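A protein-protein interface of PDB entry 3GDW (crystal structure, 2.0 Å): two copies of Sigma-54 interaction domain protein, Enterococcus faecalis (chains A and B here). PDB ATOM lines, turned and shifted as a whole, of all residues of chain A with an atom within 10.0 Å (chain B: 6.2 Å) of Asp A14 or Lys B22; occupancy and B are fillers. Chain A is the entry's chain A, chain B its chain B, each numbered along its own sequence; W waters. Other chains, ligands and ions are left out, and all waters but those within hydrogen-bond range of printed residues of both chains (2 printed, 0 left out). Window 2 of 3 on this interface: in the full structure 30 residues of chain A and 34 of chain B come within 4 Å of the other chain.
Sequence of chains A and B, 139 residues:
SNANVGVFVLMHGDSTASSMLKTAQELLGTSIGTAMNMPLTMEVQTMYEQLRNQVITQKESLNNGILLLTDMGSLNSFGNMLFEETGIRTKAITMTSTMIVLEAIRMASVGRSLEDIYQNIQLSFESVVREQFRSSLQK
OG1 of Thr B23 lies within hydrogen-bond range of O of His A12 (3.0 Å). OG of Ser B19 sits at hydrogen-bond distance from N of Asp A14, 3.4 Å away. NZ of Lys B22 is in salt-bridge range of OD2 of Asp A14 (2.6 Å). The backbone NH (N) of Ser A15 sits at hydrogen-bond distance from the side-chain hydroxyl (OG) of Ser B19, 3.0 Å away. OG1 of Thr A16 lies within hydrogen-bond range of OG of Ser B19 (2.8 Å).
N of Met A11 is in hydrogen-bond range of O of Met A36 (3.3 Å). N of Met A38 lies within hydrogen-bond range of O of Met A11 (2.8 Å). The side-chain sulfur of Met A11 sits close to the backbone NH of Asp A71, at 3.7 Å. The backbone carbonyl oxygen (O) of His A12 is in hydrogen-bond range of the side-chain hydroxyl (OG1) of Thr A16, 3.5 Å away. The backbone NH (N) of Gly A13 is in hydrogen-bond range of the backbone carbonyl oxygen (O) of Met A38 (3.0 Å). The backbone NH of Thr A16 is in hydrogen-bond range of the side-chain amide oxygen of Asn A37, at 3.5 Å.
Among the printed residues, pairs that only touch across the chains: Met A11 with Met B20 (3.8 Å), Gly A13 with Ser B19 (3.9 Å), Gly A13 with Thr B23 (3.1 Å), Thr A16 with Met B20 (3.5 Å), Leu A40 with Thr B23 (3.98 Å), Leu A40 with Glu B26 (3.5 Å) and Met A72 with Leu B27 (3.6 Å).
Printed residues of chain B within 4 Å of His A12: Thr B23. Of the printed residues of chain B, Thr A16 touches Ser B19 (2.8 Å) and Met B20 (3.5 Å). Of the printed residues of chain B, Leu A40 touches Thr B23 (3.98 Å) and Glu B26 (3.5 Å). Ser B19 touches four residues of chain A. Of the printed residues of chain A, Met B20 touches Met A11 and Thr A16. No residue of chain A comes within 4 Å of Leu B21. Of the printed residues of chain A, Lys B22 touches Asp A14. Thr B23 touches just these residues of chain A: His A12 (3.0 Å), Gly A13 (3.1 Å) and Leu A40 (3.98 Å). Of the printed residues of chain A, Glu B26 touches Leu A40. The nearest residue of chain B that does not touch Asp A14 is Thr B23 (4.8 Å). The nearest printed residue of chain B that does not touch Thr A16 is Thr B23 (4.8 Å).
Of the 23 printed residues of chain A, 8 touch a printed residue of chain B. Hydrophobic or aromatic side chains of chain A that line the printed part of chain B: Met A11, Leu A40 and Met A72. Of the 11 printed residues of chain B, 6 touch a printed residue of chain A. Hydrophobic or aromatic side chains of chain B within 4 Å of the printed part of chain A: Met B20 and Leu B27. Among the printed residues, Asp or Glu carboxylates within 4 Å of a Lys or Arg side-chain nitrogen of the other chain: Asp A14 with Lys B22.
5 positions are printed for both chains. Of the 12 pairs that touch across the chains among the printed residues, none has its exchanged pair printed and touching as well.
Water W1 bridges the side-chain carboxylate of Asp A14 and the side-chain amino group of Lys B22. Water W2 lies within hydrogen-bond range of the backbone NH (N) of Asp A14 (2.8 Å), the backbone carbonyl oxygen (O) of Ser B19 (2.9 Å) and the side-chain hydroxyl (OG1) of Thr B23 (3.4 Å).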
ATOM      1  N   MET A  11      24.744  10.482  -0.954  1.00  0.00           N
ATOM      2  CA  MET A  11      24.806  11.873  -1.464  1.00  0.00           C
ATOM      3  C   MET A  11      24.537  12.875  -0.343  1.00  0.00           C
ATOM      4  O   MET A  11      23.777  12.593   0.591  1.00  0.00           O
ATOM      5  CB  MET A  11      23.760  12.117  -2.553  1.00  0.00           C
ATOM      6  CG  MET A  11      23.805  11.169  -3.752  1.00  0.00           C
ATOM      7  SD  MET A  11      25.457  11.357  -4.776  1.00  0.00           S
ATOM      8  CE  MET A  11      24.909  12.846  -5.878  1.00  0.00           C
ATOM      9  N   HIS A  12      25.088  14.077  -0.490  1.00  0.00           N
ATOM     10  CA  HIS A  12      24.783  15.167   0.428  1.00  0.00           C
ATOM     11  C   HIS A  12      23.504  15.913   0.142  1.00  0.00           C
ATOM     12  O   HIS A  12      23.302  16.441  -0.941  1.00  0.00           O
ATOM     13  CB  HIS A  12      25.951  16.137   0.473  1.00  0.00           C
ATOM     14  CG  HIS A  12      27.143  15.550   1.130  1.00  0.00           C
ATOM     15  ND1 HIS A  12      27.176  15.280   2.481  1.00  0.00           N
ATOM     16  CD2 HIS A  12      28.312  15.096   0.619  1.00  0.00           C
ATOM     17  CE1 HIS A  12      28.327  14.701   2.779  1.00  0.00           C
ATOM     18  NE2 HIS A  12      29.042  14.597   1.671  1.00  0.00           N
ATOM     19  N   GLY A  13      22.647  15.997   1.143  1.00  0.00           N
ATOM     20  CA  GLY A  13      21.440  16.786   1.023  1.00  0.00           C
ATOM     21  C   GLY A  13      20.238  16.038   1.541  1.00  0.00           C
ATOM     22  O   GLY A  13      20.347  14.884   1.968  1.00  0.00           O
ATOM     23  N   ASP A  14      19.089  16.696   1.483  1.00  0.00           N
ATOM     24  CA  ASP A  14      17.858  16.158   2.017  1.00  0.00           C
ATOM     25  C   ASP A  14      17.369  14.927   1.278  1.00  0.00           C
ATOM     26  O   ASP A  14      16.915  13.976   1.913  1.00  0.00           O
ATOM     27  CB  ASP A  14      16.750  17.205   1.952  1.00  0.00           C
ATOM     28  CG  ASP A  14      16.909  18.309   2.968  1.00  0.00           C
ATOM     29  OD1 ASP A  14      17.862  18.272   3.774  1.00  0.00           O
ATOM     30  OD2 ASP A  14      16.056  19.224   2.953  1.00  0.00           O
ATOM     31  N   SER A  15      17.451  14.942  -0.057  1.00  0.00           N
ATOM     32  CA  SER A  15      16.831  13.871  -0.863  1.00  0.00           C
ATOM     33  C   SER A  15      17.530  13.577  -2.191  1.00  0.00           C
ATOM     34  O   SER A  15      16.918  13.027  -3.118  1.00  0.00           O
ATOM     35  CB  SER A  15      15.366  14.240  -1.147  1.00  0.00           C
ATOM     36  OG  SER A  15      15.311  15.502  -1.794  1.00  0.00           O
ATOM     37  N   THR A  16      18.790  13.974  -2.308  1.00  0.00           N
ATOM     38  CA  THR A  16      19.505  13.779  -3.555  1.00  0.00           C
ATOM     39  C   THR A  16      19.667  12.301  -3.924  1.00  0.00           C
ATOM     40  O   THR A  16      19.315  11.921  -5.034  1.00  0.00           O
ATOM     41  CB  THR A  16      20.865  14.458  -3.525  1.00  0.00           C
ATOM     42  OG1 THR A  16      20.695  15.840  -3.144  1.00  0.00           O
ATOM     43  CG2 THR A  16      21.521  14.372  -4.903  1.00  0.00           C
ATOM     44  N   ALA A  17      20.185  11.496  -2.994  1.00  0.00           N
ATOM     45  CA  ALA A  17      20.345  10.047  -3.188  1.00  0.00           C
ATOM     46  C   ALA A  17      19.008   9.341  -3.433  1.00  0.00           C
ATOM     47  O   ALA A  17      18.857   8.578  -4.396  1.00  0.00           O
ATOM     48  CB  ALA A  17      21.061   9.416  -1.955  1.00  0.00           C
ATOM     49  N   SER A  18      18.053   9.546  -2.530  1.00  0.00           N
ATOM     50  CA  SER A  18      16.742   8.873  -2.660  1.00  0.00           C
ATOM     51  C   SER A  18      16.003   9.291  -3.945  1.00  0.00           C
ATOM     52  O   SER A  18      15.410   8.442  -4.638  1.00  0.00           O
ATOM     53  CB  SER A  18      15.870   9.067  -1.404  1.00  0.00           C
ATOM     54  OG  SER A  18      15.725  10.444  -1.109  1.00  0.00           O
ATOM     55  N   SER A  19      16.051  10.578  -4.292  1.00  0.00           N
ATOM     56  CA  SER A  19      15.458  11.003  -5.576  1.00  0.00           C
ATOM     57  C   SER A  19      16.094  10.374  -6.819  1.00  0.00           C
ATOM     58  O   SER A  19      15.378   9.994  -7.758  1.00  0.00           O
ATOM     59  CB  SER A  19      15.430  12.524  -5.742  1.00  0.00           C
ATOM     60  OG  SER A  19      14.887  12.849  -7.014  1.00  0.00           O
ATOM     61  N   MET A  20      17.426  10.289  -6.844  1.00  0.00           N
ATOM     62  CA  MET A  20      18.093   9.679  -7.985  1.00  0.00           C
ATOM     63  C   MET A  20      17.767   8.194  -8.037  1.00  0.00           C
ATOM     64  O   MET A  20      17.479   7.665  -9.114  1.00  0.00           O
ATOM     65  CB  MET A  20      19.618   9.874  -7.969  1.00  0.00           C
ATOM     66  CG  MET A  20      20.110  11.288  -8.215  1.00  0.00           C
ATOM     67  SD  MET A  20      22.052  11.231  -8.374  1.00  0.00           S
ATOM     68  CE  MET A  20      22.364  10.448  -6.667  1.00  0.00           C
ATOM     69  N   LYS A  22      15.103   6.657  -6.822  1.00  0.00           N
ATOM     70  CA  LYS A  22      13.706   6.495  -7.213  1.00  0.00           C
ATOM     71  C   LYS A  22      13.504   6.653  -8.717  1.00  0.00           C
ATOM     72  O   LYS A  22      12.763   5.871  -9.327  1.00  0.00           O
ATOM     73  CB  LYS A  22      12.779   7.421  -6.408  1.00  0.00           C
ATOM     74  CG  LYS A  22      12.361   6.814  -5.079  1.00  0.00           C
ATOM     75  CD  LYS A  22      11.414   7.698  -4.294  1.00  0.00           C
ATOM     76  CE  LYS A  22      11.150   7.096  -2.929  1.00  0.00           C
ATOM     77  NZ  LYS A  22      12.349   7.124  -2.061  1.00  0.00           N
ATOM     78  N   ALA A  35      19.592   3.910  -0.921  1.00  0.00           N
ATOM     79  CA  ALA A  35      19.973   5.305  -0.948  1.00  0.00           C
ATOM     80  C   ALA A  35      20.146   5.768   0.486  1.00  0.00           C
ATOM     81  O   ALA A  35      19.412   5.343   1.373  1.00  0.00           O
ATOM     82  CB  ALA A  35      18.888   6.153  -1.661  1.00  0.00           C
ATOM     83  N   MET A  36      21.127   6.629   0.699  1.00  0.00           N
ATOM     84  CA  MET A  36      21.382   7.212   1.998  1.00  0.00           C
ATOM     85  C   MET A  36      21.635   8.673   1.781  1.00  0.00           C
ATOM     86  O   MET A  36      22.663   9.071   1.206  1.00  0.00           O
ATOM     87  CB  MET A  36      22.588   6.546   2.661  1.00  0.00           C
ATOM     88  CG  MET A  36      22.253   5.175   3.224  1.00  0.00           C
ATOM     89  SD  MET A  36      23.855   4.335   3.991  1.00  0.00           S
ATOM     90  CE  MET A  36      23.119   2.518   4.292  1.00  0.00           C
ATOM     91  N   ASN A  37      20.653   9.459   2.201  1.00  0.00           N
ATOM     92  CA  ASN A  37      20.708  10.905   2.119  1.00  0.00           C
ATOM     93  C   ASN A  37      21.505  11.348   3.314  1.00  0.00           C
ATOM     94  O   ASN A  37      21.097  11.085   4.432  1.00  0.00           O
ATOM     95  CB  ASN A  37      19.301  11.496   2.259  1.00  0.00           C
ATOM     96  CG  ASN A  37      18.411  11.202   1.074  1.00  0.00           C
ATOM     97  OD1 ASN A  37      18.829  11.325  -0.080  1.00  0.00           O
ATOM     98  ND2 ASN A  37      17.156  10.829   1.353  1.00  0.00           N
ATOM     99  N   MET A  38      22.611  12.047   3.101  1.00  0.00           N
ATOM    100  CA  MET A  38      23.402  12.534   4.244  1.00  0.00           C
ATOM    101  C   MET A  38      23.167  14.023   4.516  1.00  0.00           C
ATOM    102  O   MET A  38      23.586  14.871   3.735  1.00  0.00           O
ATOM    103  CB  MET A  38      24.884  12.253   4.005  1.00  0.00           C
ATOM    104  CG  MET A  38      25.203  10.786   3.539  1.00  0.00           C
ATOM    105  SD  MET A  38      24.949   9.359   4.913  1.00  0.00           S
ATOM    106  CE  MET A  38      25.796   7.901   3.903  1.00  0.00           C
ATOM    107  N   PRO A  39      22.490  14.355   5.624  1.00  0.00           N
ATOM    108  CA  PRO A  39      22.301  15.773   5.912  1.00  0.00           C
ATOM    109  C   PRO A  39      23.623  16.475   6.283  1.00  0.00           C
ATOM    110  O   PRO A  39      24.553  15.829   6.761  1.00  0.00           O
ATOM    111  CB  PRO A  39      21.339  15.780   7.121  1.00  0.00           C
ATOM    112  CG  PRO A  39      21.486  14.464   7.765  1.00  0.00           C
ATOM    113  CD  PRO A  39      21.950  13.476   6.685  1.00  0.00           C
ATOM    114  N   LEU A  40      23.682  17.780   6.059  1.00  0.00           N
ATOM    115  CA  LEU A  40      24.893  18.549   6.289  1.00  0.00           C
ATOM    116  C   LEU A  40      25.371  18.561   7.751  1.00  0.00           C
ATOM    117  O   LEU A  40      26.557  18.717   8.003  1.00  0.00           O
ATOM    118  CB  LEU A  40      24.731  19.961   5.749  1.00  0.00           C
ATOM    119  CG  LEU A  40      24.362  20.014   4.260  1.00  0.00           C
ATOM    120  CD1 LEU A  40      24.409  21.439   3.743  1.00  0.00           C
ATOM    121  CD2 LEU A  40      25.267  19.077   3.424  1.00  0.00           C
ATOM    122  N   THR A  41      24.437  18.378   8.684  1.00  0.00           N
ATOM    123  CA  THR A  41      24.718  18.213  10.118  1.00  0.00           C
ATOM    124  C   THR A  41      25.366  16.866  10.514  1.00  0.00           C
ATOM    125  O   THR A  41      25.823  16.714  11.645  1.00  0.00           O
ATOM    126  CB  THR A  41      23.400  18.311  10.925  1.00  0.00           C
ATOM    127  OG1 THR A  41      22.419  17.472  10.295  1.00  0.00           O
ATOM    128  CG2 THR A  41      22.882  19.737  10.956  1.00  0.00           C
ATOM    129  N   MET A  42      25.410  15.883   9.627  1.00  0.00           N
ATOM    130  CA  MET A  42      25.874  14.574  10.072  1.00  0.00           C
ATOM    131  C   MET A  42      27.385  14.456  10.018  1.00  0.00           C
ATOM    132  O   MET A  42      27.998  14.877   9.043  1.00  0.00           O
ATOM    133  CB  MET A  42      25.227  13.452   9.258  1.00  0.00           C
ATOM    134  CG  MET A  42      25.624  12.091   9.730  1.00  0.00           C
ATOM    135  SD  MET A  42      24.581  10.717   8.784  1.00  0.00           S
ATOM    136  CE  MET A  42      22.898  11.031   9.756  1.00  0.00           C
ATOM    137  N   MET A  47      28.062   8.905   9.163  1.00  0.00           N
ATOM    138  CA  MET A  47      27.750   8.510   7.780  1.00  0.00           C
ATOM    139  C   MET A  47      28.351   7.145   7.465  1.00  0.00           C
ATOM    140  O   MET A  47      27.659   6.278   6.894  1.00  0.00           O
ATOM    141  CB  MET A  47      28.313   9.504   6.752  1.00  0.00           C
ATOM    142  CG  MET A  47      27.841  10.957   6.896  1.00  0.00           C
ATOM    143  SD  MET A  47      28.206  12.177   5.378  1.00  0.00           S
ATOM    144  CE  MET A  47      27.141  13.662   6.042  1.00  0.00           C
ATOM    145  N   GLN A  50      26.693   4.334   9.317  1.00  0.00           N
ATOM    146  CA  GLN A  50      25.388   4.068   8.780  1.00  0.00           C
ATOM    147  C   GLN A  50      25.537   3.057   7.652  1.00  0.00           C
ATOM    148  O   GLN A  50      24.793   2.064   7.599  1.00  0.00           O
ATOM    149  CB  GLN A  50      24.752   5.366   8.289  1.00  0.00           C
ATOM    150  CG  GLN A  50      23.313   5.229   7.875  1.00  0.00           C
ATOM    151  CD  GLN A  50      22.661   6.601   7.637  1.00  0.00           C
ATOM    152  OE1 GLN A  50      22.783   7.528   8.446  1.00  0.00           O
ATOM    153  NE2 GLN A  50      21.946   6.715   6.528  1.00  0.00           N
ATOM    154  N   ASP A  71      29.017  11.518  -3.968  1.00  0.00           N
ATOM    155  CA  ASP A  71      29.212  12.802  -4.623  1.00  0.00           C
ATOM    156  C   ASP A  71      30.522  13.451  -4.181  1.00  0.00           C
ATOM    157  O   ASP A  71      31.395  13.683  -4.984  1.00  0.00           O
ATOM    158  CB  ASP A  71      28.005  13.749  -4.459  1.00  0.00           C
ATOM    159  CG  ASP A  71      27.535  13.917  -2.996  1.00  0.00           C
ATOM    160  OD1 ASP A  71      28.143  13.344  -2.057  1.00  0.00           O
ATOM    161  OD2 ASP A  71      26.533  14.656  -2.791  1.00  0.00           O
ATOM    162  N   MET A  72      30.635  13.712  -2.895  1.00  0.00           N
ATOM    163  CA  MET A  72      31.610  14.667  -2.405  1.00  0.00           C
ATOM    164  C   MET A  72      32.675  14.007  -1.624  1.00  0.00           C
ATOM    165  O   MET A  72      32.498  12.897  -1.147  1.00  0.00           O
ATOM    166  CB  MET A  72      30.953  15.704  -1.516  1.00  0.00           C
ATOM    167  CG  MET A  72      29.665  16.200  -2.071  1.00  0.00           C
ATOM    168  SD  MET A  72      29.850  18.017  -2.155  1.00  0.00           S
ATOM    169  CE  MET A  72      29.090  18.520  -0.418  1.00  0.00           C
ATOM    170  N   ALA B  17      17.465  17.855  -8.515  1.00  0.00           N
ATOM    171  CA  ALA B  17      17.987  19.188  -8.813  1.00  0.00           C
ATOM    172  C   ALA B  17      17.854  20.117  -7.595  1.00  0.00           C
ATOM    173  O   ALA B  17      18.828  20.818  -7.230  1.00  0.00           O
ATOM    174  CB  ALA B  17      17.287  19.810 -10.050  1.00  0.00           C
ATOM    175  N   SER B  18      16.658  20.140  -6.980  1.00  0.00           N
ATOM    176  CA  SER B  18      16.401  21.066  -5.883  1.00  0.00           C
ATOM    177  C   SER B  18      17.211  20.720  -4.628  1.00  0.00           C
ATOM    178  O   SER B  18      17.694  21.610  -3.944  1.00  0.00           O
ATOM    179  CB  SER B  18      14.896  21.186  -5.565  1.00  0.00           C
ATOM    180  OG  SER B  18      14.288  19.902  -5.404  1.00  0.00           O
ATOM    181  N   SER B  19      17.335  19.434  -4.328  1.00  0.00           N
ATOM    182  CA  SER B  19      18.110  18.994  -3.163  1.00  0.00           C
ATOM    183  C   SER B  19      19.610  19.276  -3.344  1.00  0.00           C
ATOM    184  O   SER B  19      20.274  19.686  -2.388  1.00  0.00           O
ATOM    185  CB  SER B  19      17.890  17.506  -2.946  1.00  0.00           C
ATOM    186  OG  SER B  19      18.575  17.048  -1.809  1.00  0.00           O
ATOM    187  N   MET B  20      20.142  19.025  -4.542  1.00  0.00           N
ATOM    188  CA  MET B  20      21.534  19.395  -4.810  1.00  0.00           C
ATOM    189  C   MET B  20      21.763  20.885  -4.673  1.00  0.00           C
ATOM    190  O   MET B  20      22.788  21.286  -4.109  1.00  0.00           O
ATOM    191  CB  MET B  20      21.987  19.006  -6.214  1.00  0.00           C
ATOM    192  CG  MET B  20      22.436  17.638  -6.367  1.00  0.00           C
ATOM    193  SD  MET B  20      23.123  17.433  -8.189  1.00  0.00           S
ATOM    194  CE  MET B  20      23.274  15.515  -8.062  1.00  0.00           C
ATOM    195  N   LEU B  21      20.828  21.691  -5.201  1.00  0.00           N
ATOM    196  CA  LEU B  21      20.947  23.160  -5.094  1.00  0.00           C
ATOM    197  C   LEU B  21      20.848  23.636  -3.638  1.00  0.00           C
ATOM    198  O   LEU B  21      21.609  24.520  -3.224  1.00  0.00           O
ATOM    199  CB  LEU B  21      19.910  23.902  -5.969  1.00  0.00           C
ATOM    200  CG  LEU B  21      19.964  25.441  -5.977  1.00  0.00           C
ATOM    201  CD1 LEU B  21      21.308  25.936  -6.484  1.00  0.00           C
ATOM    202  CD2 LEU B  21      18.822  26.051  -6.816  1.00  0.00           C
ATOM    203  N   LYS B  22      19.918  23.059  -2.884  1.00  0.00           N
ATOM    204  CA  LYS B  22      19.769  23.418  -1.480  1.00  0.00           C
ATOM    205  C   LYS B  22      21.085  23.157  -0.741  1.00  0.00           C
ATOM    206  O   LYS B  22      21.570  24.009  -0.014  1.00  0.00           O
ATOM    207  CB  LYS B  22      18.608  22.641  -0.850  1.00  0.00           C
ATOM    208  CG  LYS B  22      18.413  22.912   0.650  1.00  0.00           C
ATOM    209  CD  LYS B  22      17.063  22.333   1.071  1.00  0.00           C
ATOM    210  CE  LYS B  22      16.752  22.504   2.556  1.00  0.00           C
ATOM    211  NZ  LYS B  22      15.501  21.775   2.962  1.00  0.00           N
ATOM    212  N   THR B  23      21.683  21.993  -0.979  1.00  0.00           N
ATOM    213  CA  THR B  23      23.006  21.669  -0.420  1.00  0.00           C
ATOM    214  C   THR B  23      24.078  22.730  -0.719  1.00  0.00           C
ATOM    215  O   THR B  23      24.758  23.220   0.205  1.00  0.00           O
ATOM    216  CB  THR B  23      23.474  20.293  -0.937  1.00  0.00           C
ATOM    217  OG1 THR B  23      22.648  19.284  -0.353  1.00  0.00           O
ATOM    218  CG2 THR B  23      24.947  20.016  -0.553  1.00  0.00           C
ATOM    219  N   ALA B  24      24.223  23.108  -1.989  1.00  0.00           N
ATOM    220  CA  ALA B  24      25.184  24.152  -2.344  1.00  0.00           C
ATOM    221  C   ALA B  24      24.844  25.462  -1.649  1.00  0.00           C
ATOM    222  O   ALA B  24      25.736  26.140  -1.117  1.00  0.00           O
ATOM    223  CB  ALA B  24      25.255  24.360  -3.889  1.00  0.00           C
ATOM    224  N   GLN B  25      23.561  25.810  -1.650  1.00  0.00           N
ATOM    225  CA  GLN B  25      23.120  27.082  -1.101  1.00  0.00           C
ATOM    226  C   GLN B  25      23.394  27.196   0.402  1.00  0.00           C
ATOM    227  O   GLN B  25      23.780  28.273   0.888  1.00  0.00           O
ATOM    228  CB  GLN B  25      21.645  27.306  -1.382  1.00  0.00           C
ATOM    229  CG  GLN B  25      21.353  27.662  -2.833  1.00  0.00           C
ATOM    230  CD  GLN B  25      19.876  27.804  -3.075  1.00  0.00           C
ATOM    231  OE1 GLN B  25      19.057  27.327  -2.286  1.00  0.00           O
ATOM    232  NE2 GLN B  25      19.520  28.436  -4.177  1.00  0.00           N
ATOM    233  N   GLU B  26      23.176  26.093   1.116  1.00  0.00           N
ATOM    234  CA  GLU B  26      23.435  26.024   2.544  1.00  0.00           C
ATOM    235  C   GLU B  26      24.927  25.987   2.819  1.00  0.00           C
ATOM    236  O   GLU B  26      25.369  26.643   3.739  1.00  0.00           O
ATOM    237  CB  GLU B  26      22.732  24.823   3.193  1.00  0.00           C
ATOM    238  CG  GLU B  26      21.221  24.970   3.238  1.00  0.00           C
ATOM    239  CD  GLU B  26      20.497  23.720   3.754  1.00  0.00           C
ATOM    240  OE1 GLU B  26      21.163  22.720   4.116  1.00  0.00           O
ATOM    241  OE2 GLU B  26      19.244  23.736   3.795  1.00  0.00           O
ATOM    242  N   LEU B  27      25.709  25.265   2.006  1.00  0.00           N
ATOM    243  CA  LEU B  27      27.164  25.303   2.166  1.00  0.00           C
ATOM    244  C   LEU B  27      27.741  26.700   1.927  1.00  0.00           C
ATOM    245  O   LEU B  27      28.650  27.093   2.624  1.00  0.00           O
ATOM    246  CB  LEU B  27      27.892  24.269   1.289  1.00  0.00           C
ATOM    247  CG  LEU B  27      27.677  22.821   1.753  1.00  0.00           C
ATOM    248  CD1 LEU B  27      28.244  21.853   0.709  1.00  0.00           C
ATOM    249  CD2 LEU B  27      28.261  22.578   3.154  1.00  0.00           C
HETATM  250  O   HOH W   1      17.514  20.365   5.346  1.00  0.00           O
HETATM  251  O   HOH W   2      19.313  19.215   0.317  1.00  0.00           O
